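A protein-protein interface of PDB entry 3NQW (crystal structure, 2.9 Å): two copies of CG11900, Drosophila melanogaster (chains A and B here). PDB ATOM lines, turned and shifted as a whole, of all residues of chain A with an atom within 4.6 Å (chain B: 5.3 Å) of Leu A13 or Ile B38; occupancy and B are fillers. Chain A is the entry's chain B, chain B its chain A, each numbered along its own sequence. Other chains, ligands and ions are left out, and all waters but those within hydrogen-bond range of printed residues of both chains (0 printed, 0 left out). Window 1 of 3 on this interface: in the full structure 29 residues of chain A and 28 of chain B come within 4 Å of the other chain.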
ATOM      1  N   PHE A   9      22.297 -17.438  15.191  1.00  0.00           N
ATOM      2  CA  PHE A   9      23.516 -16.783  15.665  1.00  0.00           C
ATOM      3  C   PHE A   9      23.265 -15.405  16.303  1.00  0.00           C
ATOM      4  O   PHE A   9      23.991 -14.957  17.199  1.00  0.00           O
ATOM      5  CB  PHE A   9      24.507 -16.640  14.520  1.00  0.00           C
ATOM      6  CG  PHE A   9      25.795 -16.013  14.931  1.00  0.00           C
ATOM      7  CD1 PHE A   9      25.943 -14.623  14.944  1.00  0.00           C
ATOM      8  CD2 PHE A   9      26.859 -16.807  15.322  1.00  0.00           C
ATOM      9  CE1 PHE A   9      27.148 -14.034  15.340  1.00  0.00           C
ATOM     10  CE2 PHE A   9      28.065 -16.242  15.719  1.00  0.00           C
ATOM     11  CZ  PHE A   9      28.215 -14.850  15.729  1.00  0.00           C
ATOM     12  N   MET A  10      22.225 -14.742  15.825  1.00  0.00           N
ATOM     13  CA  MET A  10      21.873 -13.447  16.341  1.00  0.00           C
ATOM     14  C   MET A  10      21.109 -13.660  17.642  1.00  0.00           C
ATOM     15  O   MET A  10      21.251 -12.883  18.590  1.00  0.00           O
ATOM     16  CB  MET A  10      21.043 -12.695  15.307  1.00  0.00           C
ATOM     17  CG  MET A  10      21.761 -12.504  13.960  1.00  0.00           C
ATOM     18  SD  MET A  10      23.373 -11.707  14.122  1.00  0.00           S
ATOM     19  CE  MET A  10      22.907 -10.053  14.468  1.00  0.00           C
ATOM     20  N   GLU A  11      20.303 -14.722  17.696  1.00  0.00           N
ATOM     21  CA  GLU A  11      19.553 -15.046  18.907  1.00  0.00           C
ATOM     22  C   GLU A  11      20.544 -15.502  19.985  1.00  0.00           C
ATOM     23  O   GLU A  11      20.252 -15.422  21.180  1.00  0.00           O
ATOM     24  CB  GLU A  11      18.524 -16.143  18.618  1.00  0.00           C
ATOM     25  CG  GLU A  11      17.907 -16.755  19.869  1.00  0.00           C
ATOM     26  CD  GLU A  11      16.780 -17.727  19.560  1.00  0.00           C
ATOM     27  OE1 GLU A  11      15.781 -17.283  18.952  1.00  0.00           O
ATOM     28  OE2 GLU A  11      16.887 -18.924  19.920  1.00  0.00           O
ATOM     29  N   CYS A  12      21.710 -15.979  19.553  1.00  0.00           N
ATOM     30  CA  CYS A  12      22.758 -16.402  20.487  1.00  0.00           C
ATOM     31  C   CYS A  12      23.575 -15.180  20.946  1.00  0.00           C
ATOM     32  O   CYS A  12      23.916 -15.043  22.127  1.00  0.00           O
ATOM     33  CB  CYS A  12      23.703 -17.420  19.833  1.00  0.00           C
ATOM     34  SG  CYS A  12      25.172 -17.798  20.853  1.00  0.00           S
ATOM     35  N   LEU A  13      23.904 -14.309  19.995  1.00  0.00           N
ATOM     36  CA  LEU A  13      24.657 -13.093  20.290  1.00  0.00           C
ATOM     37  C   LEU A  13      23.802 -12.273  21.240  1.00  0.00           C
ATOM     38  O   LEU A  13      24.298 -11.715  22.210  1.00  0.00           O
ATOM     39  CB  LEU A  13      24.888 -12.273  19.017  1.00  0.00           C
ATOM     40  CG  LEU A  13      25.931 -11.148  18.929  1.00  0.00           C
ATOM     41  CD1 LEU A  13      25.337 -10.021  18.106  1.00  0.00           C
ATOM     42  CD2 LEU A  13      26.347 -10.651  20.297  1.00  0.00           C
ATOM     43  N   GLN A  14      22.508 -12.212  20.942  1.00  0.00           N
ATOM     44  CA  GLN A  14      21.569 -11.451  21.745  1.00  0.00           C
ATOM     45  C   GLN A  14      21.474 -12.038  23.124  1.00  0.00           C
ATOM     46  O   GLN A  14      21.373 -11.326  24.116  1.00  0.00           O
ATOM     47  CB  GLN A  14      20.186 -11.462  21.099  1.00  0.00           C
ATOM     48  CG  GLN A  14      19.123 -10.800  21.951  1.00  0.00           C
ATOM     49  CD  GLN A  14      17.808 -10.576  21.206  1.00  0.00           C
ATOM     50  OE1 GLN A  14      17.253 -11.490  20.583  1.00  0.00           O
ATOM     51  NE2 GLN A  14      17.294  -9.358  21.289  1.00  0.00           N
ATOM     52  N   TYR A  15      21.512 -13.356  23.177  1.00  0.00           N
ATOM     53  CA  TYR A  15      21.413 -14.060  24.436  1.00  0.00           C
ATOM     54  C   TYR A  15      22.620 -13.760  25.337  1.00  0.00           C
ATOM     55  O   TYR A  15      22.459 -13.319  26.476  1.00  0.00           O
ATOM     56  CB  TYR A  15      21.282 -15.541  24.120  1.00  0.00           C
ATOM     57  CG  TYR A  15      21.079 -16.412  25.309  1.00  0.00           C
ATOM     58  CD1 TYR A  15      22.144 -16.735  26.146  1.00  0.00           C
ATOM     59  CD2 TYR A  15      19.823 -16.946  25.591  1.00  0.00           C
ATOM     60  CE1 TYR A  15      21.963 -17.575  27.230  1.00  0.00           C
ATOM     61  CE2 TYR A  15      19.631 -17.784  26.669  1.00  0.00           C
ATOM     62  CZ  TYR A  15      20.704 -18.095  27.484  1.00  0.00           C
ATOM     63  OH  TYR A  15      20.511 -18.933  28.552  1.00  0.00           O
ATOM     64  N   ALA A  16      23.825 -13.988  24.827  1.00  0.00           N
ATOM     65  CA  ALA A  16      25.016 -13.713  25.617  1.00  0.00           C
ATOM     66  C   ALA A  16      25.008 -12.250  26.094  1.00  0.00           C
ATOM     67  O   ALA A  16      25.376 -11.950  27.221  1.00  0.00           O
ATOM     68  CB  ALA A  16      26.261 -13.998  24.797  1.00  0.00           C
ATOM     69  N   ALA A  17      24.576 -11.346  25.222  1.00  0.00           N
ATOM     70  CA  ALA A  17      24.523  -9.934  25.544  1.00  0.00           C
ATOM     71  C   ALA A  17      23.576  -9.707  26.707  1.00  0.00           C
ATOM     72  O   ALA A  17      23.864  -8.948  27.633  1.00  0.00           O
ATOM     73  CB  ALA A  17      24.052  -9.136  24.329  1.00  0.00           C
ATOM     74  N   ILE A  38      32.570 -11.351  22.920  1.00  0.00           N
ATOM     75  CA  ILE A  38      32.594 -10.898  21.536  1.00  0.00           C
ATOM     76  C   ILE A  38      34.047 -10.878  21.051  1.00  0.00           C
ATOM     77  O   ILE A  38      34.369 -11.480  20.025  1.00  0.00           O
ATOM     78  CB  ILE A  38      32.044  -9.480  21.387  1.00  0.00           C
ATOM     79  CG1 ILE A  38      30.568  -9.435  21.789  1.00  0.00           C
ATOM     80  CG2 ILE A  38      32.260  -9.002  19.952  1.00  0.00           C
ATOM     81  CD1 ILE A  38      29.867  -8.124  21.419  1.00  0.00           C
ATOM     82  N   LEU A  60      30.569 -17.238  21.761  1.00  0.00           N
ATOM     83  CA  LEU A  60      29.745 -16.175  22.300  1.00  0.00           C
ATOM     84  C   LEU A  60      29.242 -16.568  23.686  1.00  0.00           C
ATOM     85  O   LEU A  60      29.012 -15.707  24.530  1.00  0.00           O
ATOM     86  CB  LEU A  60      28.567 -15.878  21.366  1.00  0.00           C
ATOM     87  CG  LEU A  60      28.916 -15.019  20.143  1.00  0.00           C
ATOM     88  CD1 LEU A  60      27.723 -14.862  19.230  1.00  0.00           C
ATOM     89  CD2 LEU A  60      29.390 -13.657  20.600  1.00  0.00           C
ATOM     90  N   LEU B  13      30.925  -6.056  14.599  1.00  0.00           N
ATOM     91  CA  LEU B  13      30.282  -6.361  15.878  1.00  0.00           C
ATOM     92  C   LEU B  13      31.223  -5.893  16.974  1.00  0.00           C
ATOM     93  O   LEU B  13      30.815  -5.273  17.955  1.00  0.00           O
ATOM     94  CB  LEU B  13      30.088  -7.871  16.031  1.00  0.00           C
ATOM     95  CG  LEU B  13      28.984  -8.414  16.944  1.00  0.00           C
ATOM     96  CD1 LEU B  13      29.500  -9.666  17.628  1.00  0.00           C
ATOM     97  CD2 LEU B  13      28.569  -7.377  17.957  1.00  0.00           C
ATOM     98  N   VAL B  34      25.666  -1.411  24.183  1.00  0.00           N
ATOM     99  CA  VAL B  34      25.978  -2.389  23.146  1.00  0.00           C
ATOM    100  C   VAL B  34      24.813  -3.364  22.993  1.00  0.00           C
ATOM    101  O   VAL B  34      24.576  -3.885  21.908  1.00  0.00           O
ATOM    102  CB  VAL B  34      27.250  -3.201  23.497  1.00  0.00           C
ATOM    103  CG1 VAL B  34      27.622  -4.105  22.324  1.00  0.00           C
ATOM    104  CG2 VAL B  34      28.410  -2.245  23.852  1.00  0.00           C
ATOM    105  N   ASN B  35      24.098  -3.611  24.086  1.00  0.00           N
ATOM    106  CA  ASN B  35      22.957  -4.521  24.079  1.00  0.00           C
ATOM    107  C   ASN B  35      21.828  -3.969  23.197  1.00  0.00           C
ATOM    108  O   ASN B  35      21.034  -4.735  22.659  1.00  0.00           O
ATOM    109  CB  ASN B  35      22.458  -4.748  25.517  1.00  0.00           C
ATOM    110  CG  ASN B  35      23.407  -5.617  26.355  1.00  0.00           C
ATOM    111  OD1 ASN B  35      24.631  -5.494  26.277  1.00  0.00           O
ATOM    112  ND2 ASN B  35      22.830  -6.481  27.184  1.00  0.00           N
ATOM    113  N   HIS B  36      21.741  -2.650  23.052  1.00  0.00           N
ATOM    114  CA  HIS B  36      20.700  -2.060  22.211  1.00  0.00           C
ATOM    115  C   HIS B  36      21.037  -2.283  20.736  1.00  0.00           C
ATOM    116  O   HIS B  36      20.266  -2.908  20.007  1.00  0.00           O
ATOM    117  CB  HIS B  36      20.573  -0.557  22.504  1.00  0.00           C
ATOM    118  CG  HIS B  36      19.617   0.180  21.611  1.00  0.00           C
ATOM    119  ND1 HIS B  36      19.194  -0.306  20.386  1.00  0.00           N
ATOM    120  CD2 HIS B  36      19.075   1.418  21.717  1.00  0.00           C
ATOM    121  CE1 HIS B  36      18.448   0.601  19.784  1.00  0.00           C
ATOM    122  NE2 HIS B  36      18.362   1.660  20.572  1.00  0.00           N
ATOM    123  N   VAL B  37      22.192  -1.790  20.292  1.00  0.00           N
ATOM    124  CA  VAL B  37      22.527  -1.957  18.885  1.00  0.00           C
ATOM    125  C   VAL B  37      22.385  -3.416  18.477  1.00  0.00           C
ATOM    126  O   VAL B  37      21.879  -3.693  17.392  1.00  0.00           O
ATOM    127  CB  VAL B  37      23.929  -1.397  18.546  1.00  0.00           C
ATOM    128  CG1 VAL B  37      23.958   0.101  18.814  1.00  0.00           C
ATOM    129  CG2 VAL B  37      24.997  -2.105  19.368  1.00  0.00           C
ATOM    130  N   ILE B  38      22.796  -4.335  19.360  1.00  0.00           N
ATOM    131  CA  ILE B  38      22.666  -5.779  19.123  1.00  0.00           C
ATOM    132  C   ILE B  38      21.191  -6.117  18.923  1.00  0.00           C
ATOM    133  O   ILE B  38      20.827  -6.744  17.925  1.00  0.00           O
ATOM    134  CB  ILE B  38      23.188  -6.636  20.314  1.00  0.00           C
ATOM    135  CG1 ILE B  38      24.690  -6.483  20.472  1.00  0.00           C
ATOM    136  CG2 ILE B  38      22.890  -8.119  20.087  1.00  0.00           C
ATOM    137  CD1 ILE B  38      25.262  -7.370  21.585  1.00  0.00           C
ATOM    138  N   ASN B  39      20.330  -5.706  19.845  1.00  0.00           N
ATOM    139  CA  ASN B  39      18.921  -6.015  19.655  1.00  0.00           C
ATOM    140  C   ASN B  39      18.431  -5.592  18.263  1.00  0.00           C
ATOM    141  O   ASN B  39      17.784  -6.380  17.567  1.00  0.00           O
ATOM    142  CB  ASN B  39      18.050  -5.361  20.747  1.00  0.00           C
ATOM    143  CG  ASN B  39      18.225  -6.019  22.117  1.00  0.00           C
ATOM    144  OD1 ASN B  39      17.567  -5.650  23.089  1.00  0.00           O
ATOM    145  ND2 ASN B  39      19.116  -6.997  22.193  1.00  0.00           N
ATOM    146  N   VAL B  40      18.743  -4.358  17.855  1.00  0.00           N
ATOM    147  CA  VAL B  40      18.320  -3.864  16.534  1.00  0.00           C
ATOM    148  C   VAL B  40      18.808  -4.796  15.399  1.00  0.00           C
ATOM    149  O   VAL B  40      18.046  -5.115  14.483  1.00  0.00           O
ATOM    150  CB  VAL B  40      18.798  -2.383  16.270  1.00  0.00           C
ATOM    151  CG1 VAL B  40      18.469  -1.950  14.828  1.00  0.00           C
ATOM    152  CG2 VAL B  40      18.102  -1.442  17.249  1.00  0.00           C
ATOM    153  N   SER B  41      20.055  -5.257  15.455  1.00  0.00           N
ATOM    154  CA  SER B  41      20.516  -6.146  14.407  1.00  0.00           C
ATOM    155  C   SER B  41      19.745  -7.462  14.510  1.00  0.00           C
ATOM    156  O   SER B  41      19.176  -7.936  13.527  1.00  0.00           O
ATOM    157  CB  SER B  41      22.013  -6.398  14.516  1.00  0.00           C
ATOM    158  OG  SER B  41      22.504  -6.987  13.314  1.00  0.00           O
ATOM    159  N   THR B  42      19.699  -8.041  15.702  1.00  0.00           N
ATOM    160  CA  THR B  42      18.973  -9.294  15.891  1.00  0.00           C
ATOM    161  C   THR B  42      17.472  -9.202  15.544  1.00  0.00           C
ATOM    162  O   THR B  42      16.899 -10.165  15.022  1.00  0.00           O
ATOM    163  CB  THR B  42      19.119  -9.808  17.331  1.00  0.00           C
ATOM    164  OG1 THR B  42      20.469  -9.612  17.768  1.00  0.00           O
ATOM    165  CG2 THR B  42      18.790 -11.298  17.390  1.00  0.00           C
ATOM    166  N   ILE B  43      16.835  -8.067  15.845  1.00  0.00           N
ATOM    167  CA  ILE B  43      15.412  -7.870  15.528  1.00  0.00           C
ATOM    168  C   ILE B  43      15.187  -8.126  14.039  1.00  0.00           C
ATOM    169  O   ILE B  43      14.161  -8.673  13.648  1.00  0.00           O
ATOM    170  CB  ILE B  43      14.895  -6.394  15.803  1.00  0.00           C
ATOM    171  CG1 ILE B  43      14.660  -6.126  17.291  1.00  0.00           C
ATOM    172  CG2 ILE B  43      13.580  -6.162  15.075  1.00  0.00           C
ATOM    173  CD1 ILE B  43      14.278  -4.683  17.576  1.00  0.00           C
ATOM    174  N   LEU B  60      24.184  -2.779  13.532  1.00  0.00           N
ATOM    175  CA  LEU B  60      25.088  -2.849  14.671  1.00  0.00           C
ATOM    176  C   LEU B  60      25.754  -1.477  14.886  1.00  0.00           C
ATOM    177  O   LEU B  60      26.109  -1.100  16.011  1.00  0.00           O
ATOM    178  CB  LEU B  60      26.159  -3.927  14.442  1.00  0.00           C
ATOM    179  CG  LEU B  60      25.723  -5.377  14.702  1.00  0.00           C
ATOM    180  CD1 LEU B  60      26.831  -6.350  14.364  1.00  0.00           C
ATOM    181  CD2 LEU B  60      25.326  -5.523  16.154  1.00  0.00           C
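The backbone carbonyl oxygen of Met A10 sits close to the side-chain hydroxyl of Thr B42 (3.5 Å). O of Ala A17 lies within hydrogen-bond range of ND2 of Asn B35 (2.7 Å). ND2 of Asn B39 lies close to NE2 of Gln A14, at 3.1 Å.
Of the printed residues of chain B, Met A10 touches Ser B41 (3.3 Å) and Thr B42 (3.2 Å). Leu A13 touches just one residue of chain B: Ile B38 (3.7 Å). Printed residues of chain B within 4 Å of Ile A38: Leu B13. Of the printed residues of chain A, Leu B13 touches Ile A38 (3.7 Å). Val B34 touches none of the printed residues of chain A. Ile B38 touches just these residues of chain A: Leu A13 (3.7 Å), Gln A14 (3.9 Å) and Ala A17 (3.5 Å). Val B40 touches none of the printed residues of chain A. Printed residues of chain A within 4 Å of Ser B41: Met A10 (3.3 Å). Of the printed residues of chain A, Thr B42 touches Met A10 (3.2 Å), Glu A11 (3.8 Å) and Gln A14 (3.5 Å). The nearest residue of chain B that does not touch Leu A13 is Leu B13 (4.1 Å). The nearest printed residue of chain A that does not touch Ile B38 is Ile A38 (4.7 Å). The nearest printed residue of chain B that does not touch Met A10 is Ile B38 (5.2 Å).
O of Asn B35 is in hydrogen-bond range of ND2 of Asn B39, 3.0 Å away. O of Ile B38 is in hydrogen-bond range of OG1 of Thr B42, at 2.9 Å.
Ser B41 touches Met A10 (OG to CE, 3.3 Å). Glu A11 touches Thr B42 (N to CG2, 3.8 Å). Leu A13 touches Ile B38. CA of Gln A14 touches CG2 of Ile B38, at 3.9 Å. Thr B42 touches Gln A14. Ala A17 touches Ile B38. Ile A38 touches Leu B13 (CG2 to CD1, 3.7 Å).
Of the 12 printed residues of chain B, 6 touch a printed residue of chain A. Among the printed residues, no Asp or Glu carboxylate lies within 4 Å of a Lys or Arg side-chain nitrogen of the other chain.
Leu A13 touches Ile B38, and with the chains exchanged Ile A38 touches Leu B13. Positions printed for both chains: 13, 38 and 60.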
